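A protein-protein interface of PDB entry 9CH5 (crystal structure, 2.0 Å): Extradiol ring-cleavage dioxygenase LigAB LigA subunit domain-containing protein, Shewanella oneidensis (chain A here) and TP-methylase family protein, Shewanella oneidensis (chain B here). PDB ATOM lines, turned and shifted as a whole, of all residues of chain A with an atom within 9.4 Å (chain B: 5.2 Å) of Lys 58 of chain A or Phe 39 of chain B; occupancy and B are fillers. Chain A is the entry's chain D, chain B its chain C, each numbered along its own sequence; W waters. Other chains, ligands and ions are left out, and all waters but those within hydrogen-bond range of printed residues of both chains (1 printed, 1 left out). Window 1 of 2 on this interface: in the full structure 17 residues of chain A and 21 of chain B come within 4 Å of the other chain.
Water W1 lies within hydrogen-bond range of the side-chain hydroxyl (OG1) of Thr 16 of chain A and the backbone NH (N) of Trp 43 of chain B.
Of the printed residues of chain B, Phe 15 of chain A touches Leu 13 and Phe 39. Printed residues of chain B within 4 Å of Thr 16 of chain A: Leu 13 and Trp 43. Printed residues of chain B within 4 Å of Leu 57 of chain A: Phe 39 (3.8 Å). Printed residues of chain B within 4 Å of Lys 58 of chain A: Phe 39 (3.9 Å). Of the printed residues of chain B, Ser 61 of chain A touches Phe 39 (3.5 Å) and Arg 42 (3.1 Å). No residue of chain A comes within 4 Å of Gly 38 of chain B. Printed residues of chain A within 4 Å of Arg 42 of chain B: Ser 12 and Ser 61. The nearest printed residue of chain B that does not touch Thr 16 of chain A is Phe 39 of chain B (4.8 Å).
The side-chain carboxylate (OD1) of Asp 37 of chain B lies within hydrogen-bond range of the backbone NH (N) of Phe 39 of chain B, 3.0 Å away. The backbone carbonyl oxygen (O) of Ser 12 of chain A is in hydrogen-bond range of the side-chain hydroxyl (OG1) of Thr 16 of chain A (3.1 Å).
NH1 of Arg 42 of chain B lies within hydrogen-bond range of O of Ser 61 of chain A (3.1 Å).
Along chain A the printed residues that touch a printed residue of chain B span positions 12 to 61. Among the printed residues, 10 pairs touch across the chains. Among the printed residues, no Asp or Glu carboxylate lies within 4 Å of a Lys or Arg side-chain nitrogen of the other chain.
Among the printed residues, pairs that only touch across the chains: Ser 12 of chain A with Arg 42 of chain B, Ser 61 of chain A with Phe 39 of chain B, Phe 15 of chain A with Leu 13 of chain B, Phe 15 of chain A with Phe 39 of chain B, Leu 57 of chain A with Phe 39 of chain B, Ser 12 of chain A with Phe 39 of chain B, Thr 16 of chain A with Trp 43 of chain B, Lys 58 of chain A with Phe 39 of chain B and Thr 16 of chain A with Leu 13 of chain B.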
ATOM      1  N   LEU A  11       4.064 -14.281 -25.952  1.00  0.00           N
ATOM      2  CA  LEU A  11       3.483 -13.817 -24.701  1.00  0.00           C
ATOM      3  C   LEU A  11       2.246 -12.960 -24.950  1.00  0.00           C
ATOM      4  O   LEU A  11       1.163 -13.256 -24.448  1.00  0.00           O
ATOM      5  CB  LEU A  11       4.509 -13.021 -23.892  1.00  0.00           C
ATOM      6  CG  LEU A  11       5.172 -13.730 -22.710  1.00  0.00           C
ATOM      7  CD1 LEU A  11       6.081 -12.774 -21.953  1.00  0.00           C
ATOM      8  CD2 LEU A  11       4.125 -14.323 -21.783  1.00  0.00           C
ATOM      9  N   SER A  12       2.421 -11.896 -25.736  1.00  0.00           N
ATOM     10  CA  SER A  12       1.335 -10.949 -25.973  1.00  0.00           C
ATOM     11  C   SER A  12       0.136 -11.634 -26.617  1.00  0.00           C
ATOM     12  O   SER A  12      -1.015 -11.276 -26.338  1.00  0.00           O
ATOM     13  CB  SER A  12       1.823  -9.789 -26.844  1.00  0.00           C
ATOM     14  OG  SER A  12       0.775  -8.880 -27.125  1.00  0.00           O
ATOM     15  N   ASP A  13       0.386 -12.617 -27.489  1.00  0.00           N
ATOM     16  CA  ASP A  13      -0.717 -13.352 -28.104  1.00  0.00           C
ATOM     17  C   ASP A  13      -1.524 -14.093 -27.045  1.00  0.00           C
ATOM     18  O   ASP A  13      -2.759 -14.048 -27.040  1.00  0.00           O
ATOM     19  CB  ASP A  13      -0.187 -14.325 -29.158  1.00  0.00           C
ATOM     20  CG  ASP A  13       0.395 -13.614 -30.363  1.00  0.00           C
ATOM     21  OD1 ASP A  13      -0.244 -12.657 -30.856  1.00  0.00           O
ATOM     22  OD2 ASP A  13       1.477 -14.019 -30.833  1.00  0.00           O
ATOM     23  N   PHE A  14      -0.836 -14.798 -26.146  1.00  0.00           N
ATOM     24  CA  PHE A  14      -1.525 -15.566 -25.113  1.00  0.00           C
ATOM     25  C   PHE A  14      -2.355 -14.658 -24.214  1.00  0.00           C
ATOM     26  O   PHE A  14      -3.520 -14.954 -23.921  1.00  0.00           O
ATOM     27  CB  PHE A  14      -0.519 -16.365 -24.285  1.00  0.00           C
ATOM     28  CG  PHE A  14      -1.123 -17.043 -23.091  1.00  0.00           C
ATOM     29  CD1 PHE A  14      -2.042 -18.066 -23.252  1.00  0.00           C
ATOM     30  CD2 PHE A  14      -0.782 -16.648 -21.808  1.00  0.00           C
ATOM     31  CE1 PHE A  14      -2.606 -18.690 -22.152  1.00  0.00           C
ATOM     32  CE2 PHE A  14      -1.343 -17.268 -20.706  1.00  0.00           C
ATOM     33  CZ  PHE A  14      -2.255 -18.289 -20.879  1.00  0.00           C
ATOM     34  N   PHE A  15      -1.771 -13.538 -23.775  1.00  0.00           N
ATOM     35  CA  PHE A  15      -2.466 -12.661 -22.837  1.00  0.00           C
ATOM     36  C   PHE A  15      -3.709 -12.052 -23.474  1.00  0.00           C
ATOM     37  O   PHE A  15      -4.736 -11.879 -22.805  1.00  0.00           O
ATOM     38  CB  PHE A  15      -1.530 -11.554 -22.347  1.00  0.00           C
ATOM     39  CG  PHE A  15      -0.465 -12.021 -21.392  1.00  0.00           C
ATOM     40  CD1 PHE A  15      -0.537 -13.267 -20.790  1.00  0.00           C
ATOM     41  CD2 PHE A  15       0.601 -11.193 -21.078  1.00  0.00           C
ATOM     42  CE1 PHE A  15       0.444 -13.684 -19.907  1.00  0.00           C
ATOM     43  CE2 PHE A  15       1.584 -11.604 -20.195  1.00  0.00           C
ATOM     44  CZ  PHE A  15       1.504 -12.849 -19.609  1.00  0.00           C
ATOM     45  N   THR A  16      -3.630 -11.700 -24.760  1.00  0.00           N
ATOM     46  CA  THR A  16      -4.784 -11.112 -25.432  1.00  0.00           C
ATOM     47  C   THR A  16      -5.917 -12.123 -25.560  1.00  0.00           C
ATOM     48  O   THR A  16      -7.087 -11.783 -25.340  1.00  0.00           O
ATOM     49  CB  THR A  16      -4.372 -10.567 -26.800  1.00  0.00           C
ATOM     50  OG1 THR A  16      -3.495  -9.448 -26.614  1.00  0.00           O
ATOM     51  CG2 THR A  16      -5.584 -10.110 -27.593  1.00  0.00           C
ATOM     52  N   GLN A  17      -5.591 -13.367 -25.929  1.00  0.00           N
ATOM     53  CA  GLN A  17      -6.599 -14.423 -25.955  1.00  0.00           C
ATOM     54  C   GLN A  17      -7.197 -14.628 -24.569  1.00  0.00           C
ATOM     55  O   GLN A  17      -8.422 -14.684 -24.404  1.00  0.00           O
ATOM     56  CB  GLN A  17      -5.996 -15.731 -26.469  1.00  0.00           C
ATOM     57  CG  GLN A  17      -5.492 -15.691 -27.898  1.00  0.00           C
ATOM     58  CD  GLN A  17      -4.613 -16.884 -28.228  1.00  0.00           C
ATOM     59  OE1 GLN A  17      -4.516 -17.833 -27.447  1.00  0.00           O
ATOM     60  NE2 GLN A  17      -3.964 -16.839 -29.384  1.00  0.00           N
ATOM     61  N   LEU A  41       4.709 -20.726 -23.190  1.00  0.00           N
ATOM     62  CA  LEU A  41       5.448 -19.834 -22.305  1.00  0.00           C
ATOM     63  C   LEU A  41       6.674 -20.533 -21.725  1.00  0.00           C
ATOM     64  O   LEU A  41       6.623 -21.707 -21.355  1.00  0.00           O
ATOM     65  CB  LEU A  41       4.542 -19.333 -21.175  1.00  0.00           C
ATOM     66  CG  LEU A  41       3.683 -18.097 -21.480  1.00  0.00           C
ATOM     67  CD1 LEU A  41       2.526 -18.439 -22.403  1.00  0.00           C
ATOM     68  CD2 LEU A  41       3.182 -17.473 -20.188  1.00  0.00           C
ATOM     69  N   GLU A  44      10.951 -19.125 -17.331  1.00  0.00           N
ATOM     70  CA  GLU A  44      11.113 -17.811 -16.717  1.00  0.00           C
ATOM     71  C   GLU A  44       9.849 -16.977 -16.877  1.00  0.00           C
ATOM     72  O   GLU A  44       9.490 -16.208 -15.978  1.00  0.00           O
ATOM     73  CB  GLU A  44      12.321 -17.086 -17.310  1.00  0.00           C
ATOM     74  CG  GLU A  44      12.449 -17.192 -18.817  1.00  0.00           C
ATOM     75  CD  GLU A  44      13.283 -16.075 -19.407  1.00  0.00           C
ATOM     76  OE1 GLU A  44      14.524 -16.206 -19.439  1.00  0.00           O
ATOM     77  OE2 GLU A  44      12.693 -15.067 -19.849  1.00  0.00           O
ATOM     78  N   GLN A  45       9.165 -17.111 -18.020  1.00  0.00           N
ATOM     79  CA  GLN A  45       7.896 -16.412 -18.199  1.00  0.00           C
ATOM     80  C   GLN A  45       6.853 -16.943 -17.227  1.00  0.00           C
ATOM     81  O   GLN A  45       6.104 -16.167 -16.621  1.00  0.00           O
ATOM     82  CB  GLN A  45       7.408 -16.558 -19.641  1.00  0.00           C
ATOM     83  CG  GLN A  45       8.178 -15.721 -20.653  1.00  0.00           C
ATOM     84  CD  GLN A  45       7.822 -16.062 -22.087  1.00  0.00           C
ATOM     85  OE1 GLN A  45       7.027 -16.966 -22.342  1.00  0.00           O
ATOM     86  NE2 GLN A  45       8.418 -15.343 -23.033  1.00  0.00           N
ATOM     87  N   ALA A  48       7.747 -15.735 -13.799  1.00  0.00           N
ATOM     88  CA  ALA A  48       7.349 -14.340 -13.650  1.00  0.00           C
ATOM     89  C   ALA A  48       5.868 -14.230 -13.312  1.00  0.00           C
ATOM     90  O   ALA A  48       5.471 -13.402 -12.482  1.00  0.00           O
ATOM     91  CB  ALA A  48       7.666 -13.561 -14.927  1.00  0.00           C
ATOM     92  N   VAL A  49       5.036 -15.066 -13.940  1.00  0.00           N
ATOM     93  CA  VAL A  49       3.597 -15.006 -13.706  1.00  0.00           C
ATOM     94  C   VAL A  49       3.263 -15.456 -12.290  1.00  0.00           C
ATOM     95  O   VAL A  49       2.463 -14.819 -11.594  1.00  0.00           O
ATOM     96  CB  VAL A  49       2.850 -15.850 -14.757  1.00  0.00           C
ATOM     97  CG1 VAL A  49       1.434 -16.159 -14.292  1.00  0.00           C
ATOM     98  CG2 VAL A  49       2.836 -15.138 -16.101  1.00  0.00           C
ATOM     99  N   ASP A  53       5.600 -10.804 -11.007  1.00  0.00           N
ATOM    100  CA  ASP A  53       6.605  -9.822 -11.424  1.00  0.00           C
ATOM    101  C   ASP A  53       6.219  -9.298 -12.806  1.00  0.00           C
ATOM    102  O   ASP A  53       6.638  -9.835 -13.834  1.00  0.00           O
ATOM    103  CB  ASP A  53       8.001 -10.439 -11.425  1.00  0.00           C
ATOM    104  CG  ASP A  53       9.100  -9.391 -11.448  1.00  0.00           C
ATOM    105  OD1 ASP A  53       9.001  -8.430 -12.243  1.00  0.00           O
ATOM    106  OD2 ASP A  53      10.071  -9.530 -10.675  1.00  0.00           O
ATOM    107  N   MET A  54       5.411  -8.233 -12.826  1.00  0.00           N
ATOM    108  CA  MET A  54       4.971  -7.669 -14.097  1.00  0.00           C
ATOM    109  C   MET A  54       6.116  -6.983 -14.830  1.00  0.00           C
ATOM    110  O   MET A  54       6.135  -6.966 -16.068  1.00  0.00           O
ATOM    111  CB  MET A  54       3.832  -6.675 -13.868  1.00  0.00           C
ATOM    112  CG  MET A  54       2.610  -7.257 -13.178  1.00  0.00           C
ATOM    113  SD  MET A  54       1.897  -8.657 -14.061  1.00  0.00           S
ATOM    114  CE  MET A  54       2.271  -9.993 -12.928  1.00  0.00           C
ATOM    115  N   GLU A  55       7.067  -6.409 -14.084  1.00  0.00           N
ATOM    116  CA  GLU A  55       8.221  -5.763 -14.700  1.00  0.00           C
ATOM    117  C   GLU A  55       8.970  -6.733 -15.604  1.00  0.00           C
ATOM    118  O   GLU A  55       9.302  -6.405 -16.750  1.00  0.00           O
ATOM    119  CB  GLU A  55       9.143  -5.197 -13.623  1.00  0.00           C
ATOM    120  CG  GLU A  55      10.113  -4.145 -14.141  1.00  0.00           C
ATOM    121  CD  GLU A  55       9.406  -2.898 -14.636  1.00  0.00           C
ATOM    122  OE1 GLU A  55       8.897  -2.128 -13.792  1.00  0.00           O
ATOM    123  OE2 GLU A  55       9.355  -2.691 -15.867  1.00  0.00           O
ATOM    124  N   LYS A  56       9.254  -7.938 -15.100  1.00  0.00           N
ATOM    125  CA  LYS A  56      10.007  -8.899 -15.896  1.00  0.00           C
ATOM    126  C   LYS A  56       9.196  -9.370 -17.094  1.00  0.00           C
ATOM    127  O   LYS A  56       9.764  -9.626 -18.162  1.00  0.00           O
ATOM    128  CB  LYS A  56      10.428 -10.093 -15.039  1.00  0.00           C
ATOM    129  CG  LYS A  56      11.617 -10.867 -15.590  1.00  0.00           C
ATOM    130  CD  LYS A  56      12.813 -10.810 -14.652  1.00  0.00           C
ATOM    131  CE  LYS A  56      13.838 -11.882 -14.989  1.00  0.00           C
ATOM    132  NZ  LYS A  56      14.437 -11.682 -16.339  1.00  0.00           N
ATOM    133  N   LEU A  57       7.871  -9.463 -16.944  1.00  0.00           N
ATOM    134  CA  LEU A  57       7.032  -9.891 -18.057  1.00  0.00           C
ATOM    135  C   LEU A  57       7.114  -8.903 -19.213  1.00  0.00           C
ATOM    136  O   LEU A  57       7.170  -9.302 -20.382  1.00  0.00           O
ATOM    137  CB  LEU A  57       5.587 -10.049 -17.590  1.00  0.00           C
ATOM    138  CG  LEU A  57       5.253 -11.344 -16.841  1.00  0.00           C
ATOM    139  CD1 LEU A  57       3.842 -11.279 -16.294  1.00  0.00           C
ATOM    140  CD2 LEU A  57       5.426 -12.550 -17.749  1.00  0.00           C
ATOM    141  N   LYS A  58       7.117  -7.604 -18.903  1.00  0.00           N
ATOM    142  CA  LYS A  58       7.243  -6.595 -19.948  1.00  0.00           C
ATOM    143  C   LYS A  58       8.641  -6.621 -20.551  1.00  0.00           C
ATOM    144  O   LYS A  58       8.807  -6.450 -21.765  1.00  0.00           O
ATOM    145  CB  LYS A  58       6.913  -5.217 -19.383  1.00  0.00           C
ATOM    146  CG  LYS A  58       5.443  -5.033 -19.052  1.00  0.00           C
ATOM    147  CD  LYS A  58       5.226  -3.947 -18.017  1.00  0.00           C
ATOM    148  CE  LYS A  58       3.776  -3.910 -17.565  1.00  0.00           C
ATOM    149  NZ  LYS A  58       3.500  -2.795 -16.620  1.00  0.00           N
ATOM    150  N   THR A  59       9.656  -6.833 -19.709  1.00  0.00           N
ATOM    151  CA  THR A  59      11.007  -7.075 -20.201  1.00  0.00           C
ATOM    152  C   THR A  59      11.017  -8.243 -21.176  1.00  0.00           C
ATOM    153  O   THR A  59      11.553  -8.140 -22.286  1.00  0.00           O
ATOM    154  CB  THR A  59      11.956  -7.337 -19.032  1.00  0.00           C
ATOM    155  OG1 THR A  59      12.132  -6.130 -18.281  1.00  0.00           O
ATOM    156  CG2 THR A  59      13.313  -7.819 -19.531  1.00  0.00           C
ATOM    157  N   LEU A  60      10.428  -9.371 -20.772  1.00  0.00           N
ATOM    158  CA  LEU A  60      10.473 -10.582 -21.582  1.00  0.00           C
ATOM    159  C   LEU A  60       9.687 -10.440 -22.877  1.00  0.00           C
ATOM    160  O   LEU A  60       9.918 -11.210 -23.814  1.00  0.00           O
ATOM    161  CB  LEU A  60       9.941 -11.769 -20.774  1.00  0.00           C
ATOM    162  CG  LEU A  60      10.779 -12.153 -19.548  1.00  0.00           C
ATOM    163  CD1 LEU A  60      10.332 -13.478 -18.956  1.00  0.00           C
ATOM    164  CD2 LEU A  60      12.258 -12.175 -19.897  1.00  0.00           C
ATOM    165  N   SER A  61       8.773  -9.480 -22.953  1.00  0.00           N
ATOM    166  CA  SER A  61       8.038  -9.211 -24.179  1.00  0.00           C
ATOM    167  C   SER A  61       8.573  -7.974 -24.882  1.00  0.00           C
ATOM    168  O   SER A  61       8.048  -7.544 -25.903  1.00  0.00           O
ATOM    169  CB  SER A  61       6.539  -9.038 -23.889  1.00  0.00           C
ATOM    170  OG  SER A  61       5.754  -9.420 -25.001  1.00  0.00           O
ATOM    171  N   LEU B  13      -6.555  -6.118 -19.961  1.00  0.00           N
ATOM    172  CA  LEU B  13      -6.186  -6.290 -21.362  1.00  0.00           C
ATOM    173  C   LEU B  13      -7.330  -6.875 -22.184  1.00  0.00           C
ATOM    174  O   LEU B  13      -7.841  -7.957 -21.871  1.00  0.00           O
ATOM    175  CB  LEU B  13      -4.955  -7.193 -21.442  1.00  0.00           C
ATOM    176  CG  LEU B  13      -4.354  -7.544 -22.796  1.00  0.00           C
ATOM    177  CD1 LEU B  13      -3.973  -6.297 -23.554  1.00  0.00           C
ATOM    178  CD2 LEU B  13      -3.142  -8.423 -22.581  1.00  0.00           C
ATOM    179  N   PRO B  36      -2.371   1.435 -20.529  1.00  0.00           N
ATOM    180  CA  PRO B  36      -1.515   1.217 -19.349  1.00  0.00           C
ATOM    181  C   PRO B  36      -0.158   0.602 -19.649  1.00  0.00           C
ATOM    182  O   PRO B  36       0.764   0.785 -18.844  1.00  0.00           O
ATOM    183  CB  PRO B  36      -2.362   0.283 -18.467  1.00  0.00           C
ATOM    184  CG  PRO B  36      -3.758   0.384 -19.021  1.00  0.00           C
ATOM    185  CD  PRO B  36      -3.558   0.571 -20.485  1.00  0.00           C
ATOM    186  N   ASP B  37       0.010  -0.109 -20.761  1.00  0.00           N
ATOM    187  CA  ASP B  37       1.238  -0.864 -20.972  1.00  0.00           C
ATOM    188  C   ASP B  37       1.387  -1.211 -22.448  1.00  0.00           C
ATOM    189  O   ASP B  37       0.578  -0.811 -23.290  1.00  0.00           O
ATOM    190  CB  ASP B  37       1.249  -2.128 -20.106  1.00  0.00           C
ATOM    191  CG  ASP B  37       0.021  -2.996 -20.321  1.00  0.00           C
ATOM    192  OD1 ASP B  37      -0.266  -3.367 -21.482  1.00  0.00           O
ATOM    193  OD2 ASP B  37      -0.664  -3.316 -19.325  1.00  0.00           O
ATOM    194  N   GLY B  38       2.447  -1.971 -22.750  1.00  0.00           N
ATOM    195  CA  GLY B  38       2.749  -2.347 -24.119  1.00  0.00           C
ATOM    196  C   GLY B  38       1.946  -3.517 -24.635  1.00  0.00           C
ATOM    197  O   GLY B  38       1.787  -3.653 -25.853  1.00  0.00           O
ATOM    198  N   PHE B  39       1.446  -4.368 -23.736  1.00  0.00           N
ATOM    199  CA  PHE B  39       0.549  -5.440 -24.156  1.00  0.00           C
ATOM    200  C   PHE B  39      -0.761  -4.857 -24.667  1.00  0.00           C
ATOM    201  O   PHE B  39      -1.281  -5.272 -25.710  1.00  0.00           O
ATOM    202  CB  PHE B  39       0.274  -6.395 -22.994  1.00  0.00           C
ATOM    203  CG  PHE B  39       1.467  -7.196 -22.556  1.00  0.00           C
ATOM    204  CD1 PHE B  39       1.913  -8.277 -23.300  1.00  0.00           C
ATOM    205  CD2 PHE B  39       2.131  -6.879 -21.383  1.00  0.00           C
ATOM    206  CE1 PHE B  39       3.010  -9.016 -22.888  1.00  0.00           C
ATOM    207  CE2 PHE B  39       3.226  -7.612 -20.966  1.00  0.00           C
ATOM    208  CZ  PHE B  39       3.665  -8.681 -21.720  1.00  0.00           C
ATOM    209  N   SER B  40      -1.307  -3.887 -23.929  1.00  0.00           N
ATOM    210  CA  SER B  40      -2.521  -3.198 -24.355  1.00  0.00           C
ATOM    211  C   SER B  40      -2.298  -2.458 -25.664  1.00  0.00           C
ATOM    212  O   SER B  40      -3.207  -2.364 -26.497  1.00  0.00           O
ATOM    213  CB  SER B  40      -2.980  -2.233 -23.261  1.00  0.00           C
ATOM    214  OG  SER B  40      -4.328  -1.842 -23.450  1.00  0.00           O
ATOM    215  N   GLN B  41      -1.090  -1.925 -25.865  1.00  0.00           N
ATOM    216  CA  GLN B  41      -0.819  -1.141 -27.064  1.00  0.00           C
ATOM    217  C   GLN B  41      -0.721  -2.038 -28.291  1.00  0.00           C
ATOM    218  O   GLN B  41      -1.164  -1.658 -29.384  1.00  0.00           O
ATOM    219  CB  GLN B  41       0.467  -0.335 -26.878  1.00  0.00           C
ATOM    220  CG  GLN B  41       0.633   0.824 -27.849  1.00  0.00           C
ATOM    221  CD  GLN B  41      -0.299   1.980 -27.533  1.00  0.00           C
ATOM    222  OE1 GLN B  41      -0.468   2.356 -26.373  1.00  0.00           O
ATOM    223  NE2 GLN B  41      -0.900   2.555 -28.568  1.00  0.00           N
ATOM    224  N   ARG B  42      -0.129  -3.226 -28.131  1.00  0.00           N
ATOM    225  CA  ARG B  42      -0.079  -4.195 -29.221  1.00  0.00           C
ATOM    226  C   ARG B  42      -1.483  -4.616 -29.633  1.00  0.00           C
ATOM    227  O   ARG B  42      -1.803  -4.680 -30.827  1.00  0.00           O
ATOM    228  CB  ARG B  42       0.739  -5.417 -28.796  1.00  0.00           C
ATOM    229  CG  ARG B  42       2.247  -5.271 -28.936  1.00  0.00           C
ATOM    230  CD  ARG B  42       2.937  -6.576 -28.554  1.00  0.00           C
ATOM    231  NE  ARG B  42       4.319  -6.641 -29.013  1.00  0.00           N
ATOM    232  CZ  ARG B  42       5.375  -6.632 -28.206  1.00  0.00           C
ATOM    233  NH1 ARG B  42       5.241  -6.547 -26.891  1.00  0.00           N
ATOM    234  NH2 ARG B  42       6.594  -6.712 -28.730  1.00  0.00           N
ATOM    235  N   TRP B  43      -2.334  -4.918 -28.648  1.00  0.00           N
ATOM    236  CA  TRP B  43      -3.710  -5.314 -28.934  1.00  0.00           C
ATOM    237  C   TRP B  43      -4.442  -4.242 -29.726  1.00  0.00           C
ATOM    238  O   TRP B  43      -5.186  -4.550 -30.665  1.00  0.00           O
ATOM    239  CB  TRP B  43      -4.448  -5.607 -27.627  1.00  0.00           C
ATOM    240  CG  TRP B  43      -5.943  -5.494 -27.721  1.00  0.00           C
ATOM    241  CD1 TRP B  43      -6.816  -6.469 -28.105  1.00  0.00           C
ATOM    242  CD2 TRP B  43      -6.737  -4.339 -27.423  1.00  0.00           C
ATOM    243  NE1 TRP B  43      -8.106  -5.994 -28.064  1.00  0.00           N
ATOM    244  CE2 TRP B  43      -8.083  -4.687 -27.649  1.00  0.00           C
ATOM    245  CE3 TRP B  43      -6.440  -3.044 -26.986  1.00  0.00           C
ATOM    246  CZ2 TRP B  43      -9.130  -3.788 -27.453  1.00  0.00           C
ATOM    247  CZ3 TRP B  43      -7.479  -2.153 -26.793  1.00  0.00           C
ATOM    248  CH2 TRP B  43      -8.809  -2.529 -27.027  1.00  0.00           C
ATOM    249  N   LEU B 211      -3.381  -7.098 -16.450  1.00  0.00           N
ATOM    250  CA  LEU B 211      -3.159  -8.307 -17.226  1.00  0.00           C
ATOM    251  C   LEU B 211      -3.968  -9.465 -16.648  1.00  0.00           C
ATOM    252  O   LEU B 211      -4.228  -9.505 -15.442  1.00  0.00           O
ATOM    253  CB  LEU B 211      -1.671  -8.682 -17.249  1.00  0.00           C
ATOM    254  CG  LEU B 211      -0.749  -7.678 -17.950  1.00  0.00           C
ATOM    255  CD1 LEU B 211       0.697  -8.148 -17.903  1.00  0.00           C
ATOM    256  CD2 LEU B 211      -1.200  -7.446 -19.385  1.00  0.00           C
HETATM  257  O   HOH W   1      -2.550  -8.378 -28.867  1.00  0.00           O
